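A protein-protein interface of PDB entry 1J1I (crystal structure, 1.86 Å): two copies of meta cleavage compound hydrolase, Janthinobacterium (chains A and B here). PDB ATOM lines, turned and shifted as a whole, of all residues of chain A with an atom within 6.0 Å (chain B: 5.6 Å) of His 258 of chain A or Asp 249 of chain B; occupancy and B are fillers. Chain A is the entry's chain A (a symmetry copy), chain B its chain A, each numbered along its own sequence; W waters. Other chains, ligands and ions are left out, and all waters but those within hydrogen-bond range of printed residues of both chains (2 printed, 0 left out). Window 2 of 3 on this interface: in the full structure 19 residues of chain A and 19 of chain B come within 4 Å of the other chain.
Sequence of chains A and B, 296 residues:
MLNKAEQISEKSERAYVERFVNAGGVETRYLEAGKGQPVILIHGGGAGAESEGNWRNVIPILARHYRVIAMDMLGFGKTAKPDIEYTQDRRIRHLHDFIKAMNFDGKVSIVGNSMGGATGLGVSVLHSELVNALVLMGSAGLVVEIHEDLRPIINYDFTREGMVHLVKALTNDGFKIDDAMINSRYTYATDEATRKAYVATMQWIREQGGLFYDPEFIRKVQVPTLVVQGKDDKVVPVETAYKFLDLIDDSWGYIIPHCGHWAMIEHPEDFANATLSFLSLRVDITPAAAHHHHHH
The side-chain carboxylate (OD1) of Asp 250 of chain B sits close to a ring nitrogen (ND1) of His 258 of chain A, 3.4 Å away. The side-chain amino group (NZ) of Lys 231 of chain A is in hydrogen-bond range of the backbone carbonyl oxygen (O) of Leu 245 of chain B. NZ of Lys 231 of chain A lies within hydrogen-bond range of O of Ser 251 of chain B, at 2.7 Å. The side-chain carboxylate (OD2) of Asp 249 of chain B is in hydrogen-bond range of a ring nitrogen (NE2) of His 258 of chain A, 3.0 Å away.
The backbone carbonyl oxygen (O) of His 258 of chain A sits close to the side-chain amide nitrogen (ND2) of Asn 172 of chain A. NE2 of His 267 of chain A is in hydrogen-bond range of O of His 258 of chain A (2.8 Å). The side-chain carboxylate (OD2) of Asp 232 of chain A lies close to the backbone NH (N) of His 258 of chain A (3.1 Å). The backbone carbonyl oxygen (O) of Ile 248 of chain B lies within hydrogen-bond range of the side-chain hydroxyl (OG) of Ser 251 of chain B, at 2.7 Å. The backbone NH of Lys 231 of chain A sits at hydrogen-bond distance from the backbone carbonyl oxygen of Ile 256 of chain A (2.8 Å).
Among the printed residues, pairs that only touch across the chains: Lys 231 of chain A with Ile 248 of chain B (3.6 Å), Pro 257 of chain A with Asp 249 of chain B (3.7 Å) and Pro 257 of chain A with Ser 251 of chain B (3.3 Å).
Of the printed residues of chain B, His 258 of chain A touches Asp 249 (3.0 Å) and Asp 250 (3.1 Å). Of chain A, only Pro 257 and His 258 come within 4 Å of Asp 249 of chain B. Printed residues of chain A within 4 Å of Asp 250 of chain B: His 258 (3.1 Å). Printed residues of chain A within 4 Å of Ser 251 of chain B: Lys 231 and Pro 257. Of the printed residues of chain A, Ile 248 of chain B touches Lys 231 (3.6 Å). Cys 259 of chain A touches none of the printed residues of chain B. Val 221 of chain B touches none of the printed residues of chain A.
Hydrophobic or aromatic side chains of chain A that line the printed part of chain B: Pro 257 and His 258.
No position is printed for both chains. Of the 7 pairs that touch across the chains among the printed residues, none has its exchanged pair printed and touching as well.
Water W1 bridges O of Asp 249 of chain B and NZ of Lys 231 of chain A. Water W2 lies within hydrogen-bond range of ND1 of His 258 of chain A and OD1 of Asp 250 of chain B.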
ATOM      1  N   ASN A 172       3.675  13.562 -27.667  1.00  0.00           N
ATOM      2  CA  ASN A 172       3.241  12.270 -27.136  1.00  0.00           C
ATOM      3  C   ASN A 172       2.284  12.483 -25.962  1.00  0.00           C
ATOM      4  O   ASN A 172       2.352  13.502 -25.272  1.00  0.00           O
ATOM      5  CB  ASN A 172       4.456  11.442 -26.695  1.00  0.00           C
ATOM      6  CG  ASN A 172       5.047  11.915 -25.381  1.00  0.00           C
ATOM      7  OD1 ASN A 172       4.564  11.563 -24.305  1.00  0.00           O
ATOM      8  ND2 ASN A 172       6.097  12.723 -25.463  1.00  0.00           N
ATOM      9  N   LYS A 231       8.106   7.700 -32.752  1.00  0.00           N
ATOM     10  CA  LYS A 231       7.254   6.611 -33.201  1.00  0.00           C
ATOM     11  C   LYS A 231       5.790   7.019 -33.285  1.00  0.00           C
ATOM     12  O   LYS A 231       5.042   6.492 -34.108  1.00  0.00           O
ATOM     13  CB  LYS A 231       7.405   5.403 -32.261  1.00  0.00           C
ATOM     14  CG  LYS A 231       7.872   4.136 -32.963  1.00  0.00           C
ATOM     15  CD  LYS A 231       7.860   2.917 -32.045  1.00  0.00           C
ATOM     16  CE  LYS A 231       9.212   2.680 -31.377  1.00  0.00           C
ATOM     17  NZ  LYS A 231       9.198   1.444 -30.527  1.00  0.00           N
ATOM     18  N   ASP A 232       5.393   7.970 -32.446  1.00  0.00           N
ATOM     19  CA  ASP A 232       4.009   8.427 -32.402  1.00  0.00           C
ATOM     20  C   ASP A 232       3.755   9.764 -33.109  1.00  0.00           C
ATOM     21  O   ASP A 232       2.756  10.432 -32.850  1.00  0.00           O
ATOM     22  CB  ASP A 232       3.566   8.515 -30.943  1.00  0.00           C
ATOM     23  CG  ASP A 232       3.913   7.260 -30.163  1.00  0.00           C
ATOM     24  OD1 ASP A 232       3.487   6.167 -30.578  1.00  0.00           O
ATOM     25  OD2 ASP A 232       4.614   7.366 -29.141  1.00  0.00           O
ATOM     26  N   ILE A 256      12.565   6.867 -31.628  1.00  0.00           N
ATOM     27  CA  ILE A 256      12.206   7.089 -30.232  1.00  0.00           C
ATOM     28  C   ILE A 256      10.749   6.746 -29.918  1.00  0.00           C
ATOM     29  O   ILE A 256       9.827   7.209 -30.595  1.00  0.00           O
ATOM     30  CB  ILE A 256      12.448   8.571 -29.856  1.00  0.00           C
ATOM     31  CG1 ILE A 256      13.892   8.965 -30.181  1.00  0.00           C
ATOM     32  CG2 ILE A 256      12.145   8.807 -28.387  1.00  0.00           C
ATOM     33  CD1 ILE A 256      14.171  10.464 -29.994  1.00  0.00           C
ATOM     34  N   PRO A 257      10.523   5.919 -28.883  1.00  0.00           N
ATOM     35  CA  PRO A 257       9.156   5.540 -28.509  1.00  0.00           C
ATOM     36  C   PRO A 257       8.505   6.637 -27.665  1.00  0.00           C
ATOM     37  O   PRO A 257       9.202   7.472 -27.090  1.00  0.00           O
ATOM     38  CB  PRO A 257       9.368   4.255 -27.716  1.00  0.00           C
ATOM     39  CG  PRO A 257      10.656   4.560 -26.962  1.00  0.00           C
ATOM     40  CD  PRO A 257      11.518   5.203 -28.060  1.00  0.00           C
ATOM     41  N   HIS A 258       7.173   6.638 -27.606  1.00  0.00           N
ATOM     42  CA  HIS A 258       6.437   7.616 -26.801  1.00  0.00           C
ATOM     43  C   HIS A 258       6.942   9.018 -27.104  1.00  0.00           C
ATOM     44  O   HIS A 258       7.243   9.804 -26.204  1.00  0.00           O
ATOM     45  CB  HIS A 258       6.644   7.289 -25.327  1.00  0.00           C
ATOM     46  CG  HIS A 258       6.465   5.837 -25.013  1.00  0.00           C
ATOM     47  ND1 HIS A 258       7.341   5.132 -24.213  1.00  0.00           N
ATOM     48  CD2 HIS A 258       5.525   4.949 -25.415  1.00  0.00           C
ATOM     49  CE1 HIS A 258       6.947   3.874 -24.139  1.00  0.00           C
ATOM     50  NE2 HIS A 258       5.848   3.736 -24.857  1.00  0.00           N
ATOM     51  N   CYS A 259       7.020   9.318 -28.393  1.00  0.00           N
ATOM     52  CA  CYS A 259       7.532  10.591 -28.856  1.00  0.00           C
ATOM     53  C   CYS A 259       6.737  11.049 -30.062  1.00  0.00           C
ATOM     54  O   CYS A 259       6.487  10.272 -30.985  1.00  0.00           O
ATOM     55  CB  CYS A 259       9.008  10.415 -29.226  1.00  0.00           C
ATOM     56  SG  CYS A 259       9.858  11.894 -29.768  1.00  0.00           S
ATOM     57  N   GLY A 260       6.337  12.316 -30.042  1.00  0.00           N
ATOM     58  CA  GLY A 260       5.570  12.876 -31.135  1.00  0.00           C
ATOM     59  C   GLY A 260       6.442  13.524 -32.195  1.00  0.00           C
ATOM     60  O   GLY A 260       7.511  13.011 -32.535  1.00  0.00           O
ATOM     61  N   GLU A 266      10.057  17.254 -26.417  1.00  0.00           N
ATOM     62  CA  GLU A 266       9.466  16.195 -25.597  1.00  0.00           C
ATOM     63  C   GLU A 266      10.483  15.399 -24.776  1.00  0.00           C
ATOM     64  O   GLU A 266      10.189  14.971 -23.659  1.00  0.00           O
ATOM     65  CB  GLU A 266       8.669  15.235 -26.484  1.00  0.00           C
ATOM     66  CG  GLU A 266       7.586  15.909 -27.313  1.00  0.00           C
ATOM     67  CD  GLU A 266       6.935  14.964 -28.305  1.00  0.00           C
ATOM     68  OE1 GLU A 266       6.453  13.887 -27.883  1.00  0.00           O
ATOM     69  OE2 GLU A 266       6.903  15.299 -29.509  1.00  0.00           O
ATOM     70  N   HIS A 267      11.675  15.196 -25.332  1.00  0.00           N
ATOM     71  CA  HIS A 267      12.730  14.449 -24.654  1.00  0.00           C
ATOM     72  C   HIS A 267      14.061  15.114 -24.973  1.00  0.00           C
ATOM     73  O   HIS A 267      14.885  14.550 -25.694  1.00  0.00           O
ATOM     74  CB  HIS A 267      12.747  13.000 -25.153  1.00  0.00           C
ATOM     75  CG  HIS A 267      11.417  12.316 -25.075  1.00  0.00           C
ATOM     76  ND1 HIS A 267      10.857  11.909 -23.882  1.00  0.00           N
ATOM     77  CD2 HIS A 267      10.533  11.976 -26.041  1.00  0.00           C
ATOM     78  CE1 HIS A 267       9.686  11.345 -24.119  1.00  0.00           C
ATOM     79  NE2 HIS A 267       9.465  11.374 -25.421  1.00  0.00           N
ATOM     80  N   ARG B 219       6.218  -9.183 -28.006  1.00  0.00           N
ATOM     81  CA  ARG B 219       5.398  -8.071 -27.539  1.00  0.00           C
ATOM     82  C   ARG B 219       5.386  -7.998 -26.007  1.00  0.00           C
ATOM     83  O   ARG B 219       4.938  -7.004 -25.431  1.00  0.00           O
ATOM     84  CB  ARG B 219       3.970  -8.236 -28.068  1.00  0.00           C
ATOM     85  CG  ARG B 219       3.194  -6.937 -28.214  1.00  0.00           C
ATOM     86  CD  ARG B 219       1.755  -7.208 -28.623  1.00  0.00           C
ATOM     87  NE  ARG B 219       1.631  -7.762 -29.970  1.00  0.00           N
ATOM     88  CZ  ARG B 219       1.777  -7.058 -31.091  1.00  0.00           C
ATOM     89  NH1 ARG B 219       2.057  -5.760 -31.040  1.00  0.00           N
ATOM     90  NH2 ARG B 219       1.626  -7.651 -32.267  1.00  0.00           N
ATOM     91  N   VAL B 221       8.094  -7.993 -24.180  1.00  0.00           N
ATOM     92  CA  VAL B 221       9.279  -7.298 -23.687  1.00  0.00           C
ATOM     93  C   VAL B 221       8.810  -5.929 -23.193  1.00  0.00           C
ATOM     94  O   VAL B 221       8.361  -5.105 -23.982  1.00  0.00           O
ATOM     95  CB  VAL B 221      10.335  -7.114 -24.799  1.00  0.00           C
ATOM     96  CG1 VAL B 221      11.520  -6.326 -24.256  1.00  0.00           C
ATOM     97  CG2 VAL B 221      10.796  -8.481 -25.312  1.00  0.00           C
ATOM     98  N   LEU B 245      10.532  -2.876 -33.479  1.00  0.00           N
ATOM     99  CA  LEU B 245      10.123  -1.555 -33.010  1.00  0.00           C
ATOM    100  C   LEU B 245       8.609  -1.433 -32.873  1.00  0.00           C
ATOM    101  O   LEU B 245       8.112  -0.699 -32.025  1.00  0.00           O
ATOM    102  CB  LEU B 245      10.675  -0.472 -33.952  1.00  0.00           C
ATOM    103  CG  LEU B 245      12.199  -0.289 -33.877  1.00  0.00           C
ATOM    104  CD1 LEU B 245      12.666   0.701 -34.940  1.00  0.00           C
ATOM    105  CD2 LEU B 245      12.589   0.209 -32.491  1.00  0.00           C
ATOM    106  N   ASP B 246       7.882  -2.169 -33.705  1.00  0.00           N
ATOM    107  CA  ASP B 246       6.427  -2.163 -33.668  1.00  0.00           C
ATOM    108  C   ASP B 246       5.917  -3.022 -32.500  1.00  0.00           C
ATOM    109  O   ASP B 246       4.948  -2.671 -31.825  1.00  0.00           O
ATOM    110  CB  ASP B 246       5.887  -2.713 -34.989  1.00  0.00           C
ATOM    111  CG  ASP B 246       4.379  -2.690 -35.057  1.00  0.00           C
ATOM    112  OD1 ASP B 246       3.796  -1.585 -35.013  1.00  0.00           O
ATOM    113  OD2 ASP B 246       3.777  -3.779 -35.152  1.00  0.00           O
ATOM    114  N   LEU B 247       6.596  -4.137 -32.255  1.00  0.00           N
ATOM    115  CA  LEU B 247       6.208  -5.073 -31.200  1.00  0.00           C
ATOM    116  C   LEU B 247       6.595  -4.694 -29.775  1.00  0.00           C
ATOM    117  O   LEU B 247       5.808  -4.881 -28.847  1.00  0.00           O
ATOM    118  CB  LEU B 247       6.781  -6.453 -31.516  1.00  0.00           C
ATOM    119  CG  LEU B 247       6.292  -7.077 -32.824  1.00  0.00           C
ATOM    120  CD1 LEU B 247       7.135  -8.295 -33.148  1.00  0.00           C
ATOM    121  CD2 LEU B 247       4.815  -7.439 -32.699  1.00  0.00           C
ATOM    122  N   ILE B 248       7.807  -4.181 -29.594  1.00  0.00           N
ATOM    123  CA  ILE B 248       8.276  -3.810 -28.264  1.00  0.00           C
ATOM    124  C   ILE B 248       7.883  -2.360 -27.944  1.00  0.00           C
ATOM    125  O   ILE B 248       8.401  -1.408 -28.530  1.00  0.00           O
ATOM    126  CB  ILE B 248       9.804  -4.016 -28.172  1.00  0.00           C
ATOM    127  CG1 ILE B 248      10.133  -5.465 -28.552  1.00  0.00           C
ATOM    128  CG2 ILE B 248      10.302  -3.726 -26.753  1.00  0.00           C
ATOM    129  CD1 ILE B 248      11.619  -5.784 -28.610  1.00  0.00           C
ATOM    130  N   ASP B 249       6.960  -2.198 -27.002  1.00  0.00           N
ATOM    131  CA  ASP B 249       6.469  -0.867 -26.650  1.00  0.00           C
ATOM    132  C   ASP B 249       7.498   0.155 -26.183  1.00  0.00           C
ATOM    133  O   ASP B 249       7.399   1.332 -26.532  1.00  0.00           O
ATOM    134  CB  ASP B 249       5.373  -0.956 -25.591  1.00  0.00           C
ATOM    135  CG  ASP B 249       4.580   0.334 -25.484  1.00  0.00           C
ATOM    136  OD1 ASP B 249       3.836   0.647 -26.435  1.00  0.00           O
ATOM    137  OD2 ASP B 249       4.712   1.039 -24.468  1.00  0.00           O
ATOM    138  N   ASP B 250       8.469  -0.266 -25.382  1.00  0.00           N
ATOM    139  CA  ASP B 250       9.465   0.689 -24.914  1.00  0.00           C
ATOM    140  C   ASP B 250      10.790   0.522 -25.644  1.00  0.00           C
ATOM    141  O   ASP B 250      11.863   0.532 -25.033  1.00  0.00           O
ATOM    142  CB  ASP B 250       9.672   0.549 -23.407  1.00  0.00           C
ATOM    143  CG  ASP B 250      10.155   1.841 -22.769  1.00  0.00           C
ATOM    144  OD1 ASP B 250       9.724   2.918 -23.237  1.00  0.00           O
ATOM    145  OD2 ASP B 250      10.946   1.784 -21.802  1.00  0.00           O
ATOM    146  N   SER B 251      10.715   0.388 -26.961  1.00  0.00           N
ATOM    147  CA  SER B 251      11.925   0.211 -27.750  1.00  0.00           C
ATOM    148  C   SER B 251      12.336   1.420 -28.582  1.00  0.00           C
ATOM    149  O   SER B 251      11.505   2.098 -29.189  1.00  0.00           O
ATOM    150  CB  SER B 251      11.790  -1.005 -28.675  1.00  0.00           C
ATOM    151  OG  SER B 251      10.755  -0.838 -29.632  1.00  0.00           O
HETATM  152  O   HOH W   1       6.876   1.963 -29.020  1.00  0.00           O
HETATM  153  O   HOH W   2       9.814   5.834 -23.375  1.00  0.00           O
